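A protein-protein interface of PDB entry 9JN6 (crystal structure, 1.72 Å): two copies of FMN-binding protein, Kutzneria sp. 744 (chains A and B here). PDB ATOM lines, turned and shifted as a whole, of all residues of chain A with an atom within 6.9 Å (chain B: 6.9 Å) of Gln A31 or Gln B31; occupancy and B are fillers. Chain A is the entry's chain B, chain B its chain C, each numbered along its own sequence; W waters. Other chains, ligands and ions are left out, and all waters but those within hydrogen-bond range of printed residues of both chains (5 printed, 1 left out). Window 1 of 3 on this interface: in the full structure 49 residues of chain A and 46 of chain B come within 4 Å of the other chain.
Water W2 lies within hydrogen-bond range of OE1 of Gln B31 (2.7 Å) and OE1 of Gln A31 (2.8 Å).
Water W3 lies within hydrogen-bond range of O of Thr B90 (2.7 Å) and NE2 of Gln A31 (2.9 Å).
Water W4 bridges the backbone carbonyl oxygen of Thr A90 and the side-chain amide nitrogen of Gln B31.
Water W1 lies within hydrogen-bond range of O of Ile B44 (2.9 Å) and OE1 of Gln A118 (3.1 Å).
Water W5 bridges the backbone NH of Ile A44 (3.0 Å) and the side-chain amide oxygen of Gln B118 (3.3 Å).
Gln A31 touches its own counterpart, Gln B31.
Gln A31 touches Thr B90, and with the chains exchanged Thr A90 touches Gln B31.
Ile A44 touches Ala B33, but with the chains exchanged Ala A33 does not touch Ile B44 (4.1 Å).
His A46 touches Ser B116, and with the chains exchanged Ser A116 touches His B46.
Of the 13 pairs that touch across the chains among the printed residues, 11 have their exchanged pair printed and touching as well.
Among the printed residues, merely in contact across the chains: Gln A31 with Thr B90 (3.3 Å), Thr A90 with Gln B31 (3.4 Å), Val A88 with Ile B44 (3.7 Å), Ile A44 with Val B88 (3.7 Å), Thr A90 with Ile B44 (3.8 Å), Thr A90 with His B46 (3.9 Å), Ile A44 with Ala B33 (3.96 Å) and Ile A44 with Thr B90 (3.99 Å).
O of Gln A31 lies within hydrogen-bond range of N of Thr A90.
The backbone NH (N) of Ala A33 is in hydrogen-bond range of the backbone carbonyl oxygen (O) of Val A88 (2.8 Å).
The backbone NH of Gln B31 lies within hydrogen-bond range of the backbone carbonyl oxygen of Thr B90.
O of Val B88 sits at hydrogen-bond distance from N of Ala B33, 2.8 Å away.
The side-chain amide nitrogen (NE2) of Gln A31 lies close to the side-chain amide nitrogen (NE2) of Gln B31 (3.3 Å).
The backbone carbonyl oxygen (O) of Ile A44 sits at hydrogen-bond distance from the side-chain amide nitrogen (NE2) of Gln B118 (3.0 Å).
A ring nitrogen (NE2) of His A46 sits at hydrogen-bond distance from the side-chain hydroxyl (OG) of Ser B116 (2.9 Å).
The side-chain hydroxyl (OG) of Ser A116 lies within hydrogen-bond range of a ring nitrogen (NE2) of His B46 (3.0 Å).
The backbone carbonyl oxygen of Ile B44 lies within hydrogen-bond range of the side-chain amide nitrogen of Gln A118.
Of the 18 printed residues of chain A, 7 touch a printed residue of chain B.
Printed residues of chain A that touch a printed residue of chain B: Gln A31, Ile A44, His A46, Val A88, Thr A90, Ser A116 and Gln A118.
Hydrophobic or aromatic side chains of chain A that line the printed part of chain B: Ile A44, His A46 and Val A88.
Of the printed residues of chain A, Gln B31 touches Gln A31 (3.3 Å) and Thr A90 (3.4 Å).
Printed residues of chain A within 4 Å of Ala B33: Ile A44 (3.96 Å).
Printed residues of chain A within 4 Å of Thr B90: Gln A31 (3.3 Å) and Ile A44 (3.99 Å).
Of the printed residues of chain B, His A46 touches Ser B116.
Of the printed residues of chain A, Ile B44 touches Val A88, Thr A90 and Gln A118.
Of the printed residues of chain A, Gln B118 touches Ile A44 (3.0 Å).
The nearest residue of chain B that does not touch Gln A31 is Ala B92 (4.2 Å).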
ATOM      1  N   PRO A  28      15.690 -25.742  -4.665  1.00  0.00           N
ATOM      2  CA  PRO A  28      17.037 -25.895  -4.101  1.00  0.00           C
ATOM      3  C   PRO A  28      17.575 -24.683  -3.331  1.00  0.00           C
ATOM      4  O   PRO A  28      18.570 -24.880  -2.631  1.00  0.00           O
ATOM      5  CB  PRO A  28      17.947 -26.148  -5.300  1.00  0.00           C
ATOM      6  CG  PRO A  28      17.192 -25.522  -6.454  1.00  0.00           C
ATOM      7  CD  PRO A  28      15.713 -25.665  -6.135  1.00  0.00           C
ATOM      8  N   LEU A  29      16.981 -23.490  -3.494  1.00  0.00           N
ATOM      9  CA  LEU A  29      17.462 -22.312  -2.743  1.00  0.00           C
ATOM     10  C   LEU A  29      16.827 -22.372  -1.344  1.00  0.00           C
ATOM     11  O   LEU A  29      15.751 -21.840  -1.127  1.00  0.00           O
ATOM     12  CB  LEU A  29      17.206 -21.006  -3.491  1.00  0.00           C
ATOM     13  CG  LEU A  29      17.955 -19.801  -2.909  1.00  0.00           C
ATOM     14  CD1 LEU A  29      19.432 -19.899  -3.221  1.00  0.00           C
ATOM     15  CD2 LEU A  29      17.366 -18.453  -3.371  1.00  0.00           C
ATOM     16  N   ALA A  30      17.544 -22.987  -0.411  1.00  0.00           N
ATOM     17  CA  ALA A  30      17.100 -23.239   0.970  1.00  0.00           C
ATOM     18  C   ALA A  30      17.489 -22.094   1.883  1.00  0.00           C
ATOM     19  O   ALA A  30      18.462 -21.326   1.584  1.00  0.00           O
ATOM     20  CB  ALA A  30      17.704 -24.516   1.468  1.00  0.00           C
ATOM     21  N   GLN A  31      16.741 -21.982   2.975  1.00  0.00           N
ATOM     22  CA  GLN A  31      17.129 -21.089   4.100  1.00  0.00           C
ATOM     23  C   GLN A  31      17.888 -21.943   5.102  1.00  0.00           C
ATOM     24  O   GLN A  31      17.328 -22.901   5.705  1.00  0.00           O
ATOM     25  CB  GLN A  31      15.953 -20.381   4.745  1.00  0.00           C
ATOM     26  CG  GLN A  31      15.258 -19.440   3.772  1.00  0.00           C
ATOM     27  CD  GLN A  31      14.145 -18.644   4.430  1.00  0.00           C
ATOM     28  OE1 GLN A  31      14.216 -18.314   5.607  1.00  0.00           O
ATOM     29  NE2 GLN A  31      13.119 -18.293   3.650  1.00  0.00           N
ATOM     30  N   LEU A  32      19.171 -21.667   5.208  1.00  0.00           N
ATOM     31  CA  LEU A  32      20.034 -22.388   6.163  1.00  0.00           C
ATOM     32  C   LEU A  32      20.053 -21.581   7.468  1.00  0.00           C
ATOM     33  O   LEU A  32      20.449 -20.454   7.405  1.00  0.00           O
ATOM     34  CB  LEU A  32      21.435 -22.474   5.560  1.00  0.00           C
ATOM     35  CG  LEU A  32      22.468 -23.138   6.469  1.00  0.00           C
ATOM     36  CD1 LEU A  32      22.151 -24.594   6.647  1.00  0.00           C
ATOM     37  CD2 LEU A  32      23.879 -22.930   5.947  1.00  0.00           C
ATOM     38  N   ALA A  33      19.703 -22.199   8.582  1.00  0.00           N
ATOM     39  CA  ALA A  33      19.613 -21.572   9.902  1.00  0.00           C
ATOM     40  C   ALA A  33      20.535 -22.294  10.902  1.00  0.00           C
ATOM     41  O   ALA A  33      20.512 -23.523  10.986  1.00  0.00           O
ATOM     42  CB  ALA A  33      18.181 -21.524  10.379  1.00  0.00           C
ATOM     43  N   ILE A  44      20.546 -16.647   9.239  1.00  0.00           N
ATOM     44  CA  ILE A  44      19.766 -17.252   8.136  1.00  0.00           C
ATOM     45  C   ILE A  44      20.409 -16.835   6.818  1.00  0.00           C
ATOM     46  O   ILE A  44      20.628 -15.627   6.601  1.00  0.00           O
ATOM     47  CB  ILE A  44      18.301 -16.786   8.160  1.00  0.00           C
ATOM     48  CG1 ILE A  44      17.620 -16.930   9.525  1.00  0.00           C
ATOM     49  CG2 ILE A  44      17.549 -17.475   7.041  1.00  0.00           C
ATOM     50  CD1 ILE A  44      17.003 -18.291   9.680  1.00  0.00           C
ATOM     51  N   THR A  45      20.795 -17.812   5.991  1.00  0.00           N
ATOM     52  CA  THR A  45      21.339 -17.556   4.661  1.00  0.00           C
ATOM     53  C   THR A  45      20.609 -18.379   3.611  1.00  0.00           C
ATOM     54  O   THR A  45      20.418 -19.604   3.864  1.00  0.00           O
ATOM     55  CB  THR A  45      22.850 -17.843   4.618  1.00  0.00           C
ATOM     56  OG1 THR A  45      23.455 -17.043   5.644  1.00  0.00           O
ATOM     57  CG2 THR A  45      23.388 -17.442   3.260  1.00  0.00           C
ATOM     58  N   HIS A  46      20.231 -17.729   2.501  1.00  0.00           N
ATOM     59  CA  HIS A  46      19.736 -18.448   1.299  1.00  0.00           C
ATOM     60  C   HIS A  46      20.892 -19.069   0.556  1.00  0.00           C
ATOM     61  O   HIS A  46      21.784 -18.347   0.114  1.00  0.00           O
ATOM     62  CB  HIS A  46      18.940 -17.583   0.385  1.00  0.00           C
ATOM     63  CG  HIS A  46      17.652 -17.142   0.970  1.00  0.00           C
ATOM     64  ND1 HIS A  46      16.456 -17.674   0.629  1.00  0.00           N
ATOM     65  CD2 HIS A  46      17.414 -16.198   1.884  1.00  0.00           C
ATOM     66  CE1 HIS A  46      15.500 -17.082   1.321  1.00  0.00           C
ATOM     67  NE2 HIS A  46      16.070 -16.183   2.113  1.00  0.00           N
ATOM     68  N   VAL A  47      20.894 -20.372   0.463  1.00  0.00           N
ATOM     69  CA  VAL A  47      21.993 -21.154  -0.152  1.00  0.00           C
ATOM     70  C   VAL A  47      21.444 -22.248  -1.038  1.00  0.00           C
ATOM     71  O   VAL A  47      20.401 -22.877  -0.724  1.00  0.00           O
ATOM     72  CB  VAL A  47      22.890 -21.772   0.938  1.00  0.00           C
ATOM     73  CG1 VAL A  47      23.597 -20.699   1.747  1.00  0.00           C
ATOM     74  CG2 VAL A  47      22.127 -22.679   1.906  1.00  0.00           C
ATOM     75  N   ILE A  49      21.253 -25.810  -2.442  1.00  0.00           N
ATOM     76  CA  ILE A  49      21.533 -27.132  -1.825  1.00  0.00           C
ATOM     77  C   ILE A  49      20.977 -28.234  -2.720  1.00  0.00           C
ATOM     78  O   ILE A  49      19.826 -28.107  -3.149  1.00  0.00           O
ATOM     79  CB  ILE A  49      20.983 -27.237  -0.382  1.00  0.00           C
ATOM     80  CG1 ILE A  49      21.641 -26.217   0.552  1.00  0.00           C
ATOM     81  CG2 ILE A  49      21.154 -28.663   0.094  1.00  0.00           C
ATOM     82  CD1 ILE A  49      21.150 -26.310   1.983  1.00  0.00           C
ATOM     83  N   VAL A  88      19.512 -26.328  10.526  1.00  0.00           N
ATOM     84  CA  VAL A  88      18.266 -26.695   9.806  1.00  0.00           C
ATOM     85  C   VAL A  88      18.331 -26.018   8.432  1.00  0.00           C
ATOM     86  O   VAL A  88      18.907 -24.878   8.334  1.00  0.00           O
ATOM     87  CB  VAL A  88      16.977 -26.339  10.578  1.00  0.00           C
ATOM     88  CG1 VAL A  88      16.944 -24.881  10.961  1.00  0.00           C
ATOM     89  CG2 VAL A  88      15.749 -26.679   9.734  1.00  0.00           C
ATOM     90  N   ALA A  89      17.974 -26.752   7.391  1.00  0.00           N
ATOM     91  CA  ALA A  89      17.806 -26.168   6.023  1.00  0.00           C
ATOM     92  C   ALA A  89      16.368 -26.361   5.626  1.00  0.00           C
ATOM     93  O   ALA A  89      15.848 -27.502   5.732  1.00  0.00           O
ATOM     94  CB  ALA A  89      18.800 -26.724   5.034  1.00  0.00           C
ATOM     95  N   THR A  90      15.701 -25.244   5.339  1.00  0.00           N
ATOM     96  CA  THR A  90      14.249 -25.250   5.046  1.00  0.00           C
ATOM     97  C   THR A  90      14.072 -24.978   3.558  1.00  0.00           C
ATOM     98  O   THR A  90      14.655 -24.004   3.042  1.00  0.00           O
ATOM     99  CB  THR A  90      13.480 -24.212   5.858  1.00  0.00           C
ATOM    100  OG1 THR A  90      13.736 -24.432   7.263  1.00  0.00           O
ATOM    101  CG2 THR A  90      12.003 -24.333   5.527  1.00  0.00           C
ATOM    102  N   PHE A  91      13.285 -25.815   2.915  1.00  0.00           N
ATOM    103  CA  PHE A  91      13.009 -25.751   1.466  1.00  0.00           C
ATOM    104  C   PHE A  91      11.521 -25.432   1.377  1.00  0.00           C
ATOM    105  O   PHE A  91      10.708 -26.137   1.978  1.00  0.00           O
ATOM    106  CB  PHE A  91      13.342 -27.066   0.789  1.00  0.00           C
ATOM    107  CG  PHE A  91      14.772 -27.529   0.883  1.00  0.00           C
ATOM    108  CD1 PHE A  91      15.248 -28.131   2.041  1.00  0.00           C
ATOM    109  CD2 PHE A  91      15.664 -27.347  -0.171  1.00  0.00           C
ATOM    110  CE1 PHE A  91      16.557 -28.564   2.140  1.00  0.00           C
ATOM    111  CE2 PHE A  91      16.980 -27.760  -0.066  1.00  0.00           C
ATOM    112  CZ  PHE A  91      17.430 -28.354   1.095  1.00  0.00           C
ATOM    113  N   ALA A  92      11.164 -24.402   0.651  1.00  0.00           N
ATOM    114  CA  ALA A  92       9.778 -23.894   0.599  1.00  0.00           C
ATOM    115  C   ALA A  92       9.272 -24.107  -0.828  1.00  0.00           C
ATOM    116  O   ALA A  92       9.912 -23.604  -1.773  1.00  0.00           O
ATOM    117  CB  ALA A  92       9.771 -22.422   1.002  1.00  0.00           C
ATOM    118  N   SER A 116       6.645 -27.360   2.830  1.00  0.00           N
ATOM    119  CA  SER A 116       7.940 -27.022   3.464  1.00  0.00           C
ATOM    120  C   SER A 116       8.646 -28.328   3.807  1.00  0.00           C
ATOM    121  O   SER A 116       7.932 -29.283   4.209  1.00  0.00           O
ATOM    122  CB  SER A 116       7.710 -26.212   4.718  1.00  0.00           C
ATOM    123  OG  SER A 116       8.940 -25.936   5.319  1.00  0.00           O
ATOM    124  N   GLN A 118      11.968 -29.388   6.223  1.00  0.00           N
ATOM    125  CA  GLN A 118      13.076 -28.952   7.109  1.00  0.00           C
ATOM    126  C   GLN A 118      13.995 -30.150   7.313  1.00  0.00           C
ATOM    127  O   GLN A 118      13.524 -31.204   7.727  1.00  0.00           O
ATOM    128  CB  GLN A 118      12.572 -28.406   8.439  1.00  0.00           C
ATOM    129  CG  GLN A 118      11.769 -27.108   8.292  1.00  0.00           C
ATOM    130  CD  GLN A 118      11.203 -26.639   9.596  1.00  0.00           C
ATOM    131  OE1 GLN A 118      11.595 -27.077  10.688  1.00  0.00           O
ATOM    132  NE2 GLN A 118      10.233 -25.750   9.484  1.00  0.00           N
ATOM    133  N   PRO B  28       3.420 -12.491   3.390  1.00  0.00           N
ATOM    134  CA  PRO B  28       3.228 -12.533   4.843  1.00  0.00           C
ATOM    135  C   PRO B  28       3.515 -13.860   5.543  1.00  0.00           C
ATOM    136  O   PRO B  28       3.620 -13.850   6.767  1.00  0.00           O
ATOM    137  CB  PRO B  28       1.732 -12.179   4.999  1.00  0.00           C
ATOM    138  CG  PRO B  28       1.121 -12.595   3.707  1.00  0.00           C
ATOM    139  CD  PRO B  28       2.156 -12.326   2.643  1.00  0.00           C
ATOM    140  N   LEU B  29       3.531 -14.982   4.797  1.00  0.00           N
ATOM    141  CA  LEU B  29       3.857 -16.271   5.437  1.00  0.00           C
ATOM    142  C   LEU B  29       5.377 -16.365   5.597  1.00  0.00           C
ATOM    143  O   LEU B  29       6.095 -16.841   4.678  1.00  0.00           O
ATOM    144  CB  LEU B  29       3.266 -17.445   4.662  1.00  0.00           C
ATOM    145  CG  LEU B  29       3.255 -18.772   5.446  1.00  0.00           C
ATOM    146  CD1 LEU B  29       2.203 -18.771   6.563  1.00  0.00           C
ATOM    147  CD2 LEU B  29       3.079 -19.961   4.496  1.00  0.00           C
ATOM    148  N   ALA B  30       5.832 -15.939   6.772  1.00  0.00           N
ATOM    149  CA  ALA B  30       7.239 -15.786   7.140  1.00  0.00           C
ATOM    150  C   ALA B  30       7.743 -17.087   7.745  1.00  0.00           C
ATOM    151  O   ALA B  30       6.937 -17.847   8.253  1.00  0.00           O
ATOM    152  CB  ALA B  30       7.379 -14.635   8.099  1.00  0.00           C
ATOM    153  N   GLN B  31       9.036 -17.315   7.693  1.00  0.00           N
ATOM    154  CA  GLN B  31       9.674 -18.372   8.515  1.00  0.00           C
ATOM    155  C   GLN B  31      10.186 -17.690   9.780  1.00  0.00           C
ATOM    156  O   GLN B  31      11.155 -16.877   9.696  1.00  0.00           O
ATOM    157  CB  GLN B  31      10.777 -19.070   7.725  1.00  0.00           C
ATOM    158  CG  GLN B  31      10.290 -19.889   6.544  1.00  0.00           C
ATOM    159  CD  GLN B  31      11.364 -20.674   5.810  1.00  0.00           C
ATOM    160  OE1 GLN B  31      12.373 -21.092   6.380  1.00  0.00           O
ATOM    161  NE2 GLN B  31      11.174 -20.832   4.516  1.00  0.00           N
ATOM    162  N   LEU B  32       9.589 -18.033  10.899  1.00  0.00           N
ATOM    163  CA  LEU B  32       9.979 -17.501  12.214  1.00  0.00           C
ATOM    164  C   LEU B  32      11.023 -18.454  12.786  1.00  0.00           C
ATOM    165  O   LEU B  32      10.708 -19.663  12.917  1.00  0.00           O
ATOM    166  CB  LEU B  32       8.769 -17.395  13.118  1.00  0.00           C
ATOM    167  CG  LEU B  32       9.079 -16.947  14.562  1.00  0.00           C
ATOM    168  CD1 LEU B  32       9.623 -15.529  14.633  1.00  0.00           C
ATOM    169  CD2 LEU B  32       7.861 -17.054  15.451  1.00  0.00           C
ATOM    170  N   ALA B  33      12.230 -17.941  13.071  1.00  0.00           N
ATOM    171  CA  ALA B  33      13.309 -18.772  13.633  1.00  0.00           C
ATOM    172  C   ALA B  33      13.683 -18.289  15.039  1.00  0.00           C
ATOM    173  O   ALA B  33      13.943 -17.090  15.215  1.00  0.00           O
ATOM    174  CB  ALA B  33      14.522 -18.804  12.721  1.00  0.00           C
ATOM    175  N   ILE B  44      11.964 -23.545  13.536  1.00  0.00           N
ATOM    176  CA  ILE B  44      11.440 -22.847  12.323  1.00  0.00           C
ATOM    177  C   ILE B  44       9.953 -23.114  12.225  1.00  0.00           C
ATOM    178  O   ILE B  44       9.597 -24.294  12.114  1.00  0.00           O
ATOM    179  CB  ILE B  44      12.113 -23.353  11.030  1.00  0.00           C
ATOM    180  CG1 ILE B  44      13.627 -23.343  11.101  1.00  0.00           C
ATOM    181  CG2 ILE B  44      11.626 -22.586   9.833  1.00  0.00           C
ATOM    182  CD1 ILE B  44      14.238 -22.002  11.243  1.00  0.00           C
ATOM    183  N   THR B  45       9.131 -22.056  12.191  1.00  0.00           N
ATOM    184  CA  THR B  45       7.684 -22.227  11.948  1.00  0.00           C
ATOM    185  C   THR B  45       7.255 -21.209  10.910  1.00  0.00           C
ATOM    186  O   THR B  45       7.688 -20.048  10.962  1.00  0.00           O
ATOM    187  CB  THR B  45       6.828 -22.070  13.216  1.00  0.00           C
ATOM    188  OG1 THR B  45       7.349 -22.963  14.223  1.00  0.00           O
ATOM    189  CG2 THR B  45       5.371 -22.365  12.920  1.00  0.00           C
ATOM    190  N   HIS B  46       6.473 -21.686   9.945  1.00  0.00           N
ATOM    191  CA  HIS B  46       5.816 -20.820   8.937  1.00  0.00           C
ATOM    192  C   HIS B  46       4.610 -20.144   9.595  1.00  0.00           C
ATOM    193  O   HIS B  46       3.679 -20.819  10.004  1.00  0.00           O
ATOM    194  CB  HIS B  46       5.438 -21.598   7.674  1.00  0.00           C
ATOM    195  CG  HIS B  46       6.610 -22.075   6.866  1.00  0.00           C
ATOM    196  ND1 HIS B  46       7.038 -21.421   5.742  1.00  0.00           N
ATOM    197  CD2 HIS B  46       7.469 -23.087   7.058  1.00  0.00           C
ATOM    198  CE1 HIS B  46       8.087 -22.033   5.247  1.00  0.00           C
ATOM    199  NE2 HIS B  46       8.358 -23.080   6.018  1.00  0.00           N
ATOM    200  N   VAL B  47       4.653 -18.838   9.712  1.00  0.00           N
ATOM    201  CA  VAL B  47       3.604 -18.067  10.423  1.00  0.00           C
ATOM    202  C   VAL B  47       3.190 -16.853   9.606  1.00  0.00           C
ATOM    203  O   VAL B  47       4.052 -16.161   9.047  1.00  0.00           O
ATOM    204  CB  VAL B  47       4.049 -17.647  11.826  1.00  0.00           C
ATOM    205  CG1 VAL B  47       4.227 -18.827  12.764  1.00  0.00           C
ATOM    206  CG2 VAL B  47       5.362 -16.838  11.785  1.00  0.00           C
ATOM    207  N   ILE B  49       2.508 -13.124   9.330  1.00  0.00           N
ATOM    208  CA  ILE B  49       2.927 -11.887  10.011  1.00  0.00           C
ATOM    209  C   ILE B  49       2.483 -10.695   9.174  1.00  0.00           C
ATOM    210  O   ILE B  49       2.670 -10.682   7.943  1.00  0.00           O
ATOM    211  CB  ILE B  49       4.420 -11.908  10.310  1.00  0.00           C
ATOM    212  CG1 ILE B  49       4.750 -13.093  11.230  1.00  0.00           C
ATOM    213  CG2 ILE B  49       4.788 -10.571  10.922  1.00  0.00           C
ATOM    214  CD1 ILE B  49       6.246 -13.299  11.516  1.00  0.00           C
ATOM    215  N   VAL B  88      14.335 -14.134  14.564  1.00  0.00           N
ATOM    216  CA  VAL B  88      14.355 -13.604  13.180  1.00  0.00           C
ATOM    217  C   VAL B  88      13.117 -14.085  12.449  1.00  0.00           C
ATOM    218  O   VAL B  88      12.714 -15.263  12.627  1.00  0.00           O
ATOM    219  CB  VAL B  88      15.643 -13.963  12.417  1.00  0.00           C
ATOM    220  CG1 VAL B  88      15.940 -15.451  12.462  1.00  0.00           C
ATOM    221  CG2 VAL B  88      15.570 -13.469  10.983  1.00  0.00           C
ATOM    222  N   ALA B  89      12.539 -13.216  11.630  1.00  0.00           N
ATOM    223  CA  ALA B  89      11.414 -13.624  10.752  1.00  0.00           C
ATOM    224  C   ALA B  89      11.832 -13.284   9.338  1.00  0.00           C
ATOM    225  O   ALA B  89      12.280 -12.130   9.096  1.00  0.00           O
ATOM    226  CB  ALA B  89      10.114 -12.949  11.091  1.00  0.00           C
ATOM    227  N   THR B  90      11.798 -14.293   8.486  1.00  0.00           N
ATOM    228  CA  THR B  90      12.295 -14.198   7.104  1.00  0.00           C
ATOM    229  C   THR B  90      11.100 -14.257   6.156  1.00  0.00           C
ATOM    230  O   THR B  90      10.242 -15.228   6.211  1.00  0.00           O
ATOM    231  CB  THR B  90      13.332 -15.262   6.759  1.00  0.00           C
ATOM    232  OG1 THR B  90      14.374 -15.159   7.728  1.00  0.00           O
ATOM    233  CG2 THR B  90      13.842 -15.073   5.341  1.00  0.00           C
ATOM    234  N   PHE B  91      11.029 -13.239   5.333  1.00  0.00           N
ATOM    235  CA  PHE B  91      10.020 -13.092   4.263  1.00  0.00           C
ATOM    236  C   PHE B  91      10.742 -13.261   2.931  1.00  0.00           C
ATOM    237  O   PHE B  91      11.743 -12.582   2.644  1.00  0.00           O
ATOM    238  CB  PHE B  91       9.319 -11.742   4.330  1.00  0.00           C
ATOM    239  CG  PHE B  91       8.691 -11.416   5.672  1.00  0.00           C
ATOM    240  CD1 PHE B  91       9.478 -11.008   6.730  1.00  0.00           C
ATOM    241  CD2 PHE B  91       7.307 -11.478   5.890  1.00  0.00           C
ATOM    242  CE1 PHE B  91       8.925 -10.660   7.937  1.00  0.00           C
ATOM    243  CE2 PHE B  91       6.759 -11.083   7.093  1.00  0.00           C
ATOM    244  CZ  PHE B  91       7.563 -10.798   8.156  1.00  0.00           C
ATOM    245  N   ALA B  92      10.183 -14.095   2.093  1.00  0.00           N
ATOM    246  CA  ALA B  92      10.786 -14.474   0.809  1.00  0.00           C
ATOM    247  C   ALA B  92       9.869 -14.059  -0.315  1.00  0.00           C
ATOM    248  O   ALA B  92       8.753 -14.608  -0.390  1.00  0.00           O
ATOM    249  CB  ALA B  92      11.045 -15.958   0.784  1.00  0.00           C
ATOM    250  N   SER B 116      14.623 -11.303  -0.261  1.00  0.00           N
ATOM    251  CA  SER B 116      14.407 -11.713   1.138  1.00  0.00           C
ATOM    252  C   SER B 116      14.357 -10.478   2.004  1.00  0.00           C
ATOM    253  O   SER B 116      15.183  -9.611   1.830  1.00  0.00           O
ATOM    254  CB  SER B 116      15.526 -12.653   1.549  1.00  0.00           C
ATOM    255  OG  SER B 116      15.211 -13.427   2.677  1.00  0.00           O
ATOM    256  N   GLN B 118      14.792 -10.084   6.223  1.00  0.00           N
ATOM    257  CA  GLN B 118      15.003 -10.628   7.568  1.00  0.00           C
ATOM    258  C   GLN B 118      14.789  -9.530   8.579  1.00  0.00           C
ATOM    259  O   GLN B 118      15.520  -8.505   8.544  1.00  0.00           O
ATOM    260  CB  GLN B 118      16.353 -11.279   7.772  1.00  0.00           C
ATOM    261  CG  GLN B 118      16.540 -12.460   6.873  1.00  0.00           C
ATOM    262  CD  GLN B 118      17.902 -13.076   7.067  1.00  0.00           C
ATOM    263  OE1 GLN B 118      18.566 -12.872   8.070  1.00  0.00           O
ATOM    264  NE2 GLN B 118      18.299 -13.877   6.108  1.00  0.00           N
HETATM  265  O   HOH W   1      10.951 -26.361  13.638  1.00  0.00           O
HETATM  266  O   HOH W   2      14.330 -19.940   7.880  1.00  0.00           O
HETATM  267  O   HOH W   3      10.549 -17.005   4.146  1.00  0.00           O
HETATM  268  O   HOH W   4      12.856 -21.897   2.490  1.00  0.00           O
HETATM  269  O   HOH W   5      21.598 -13.868   9.003  1.00  0.00           O
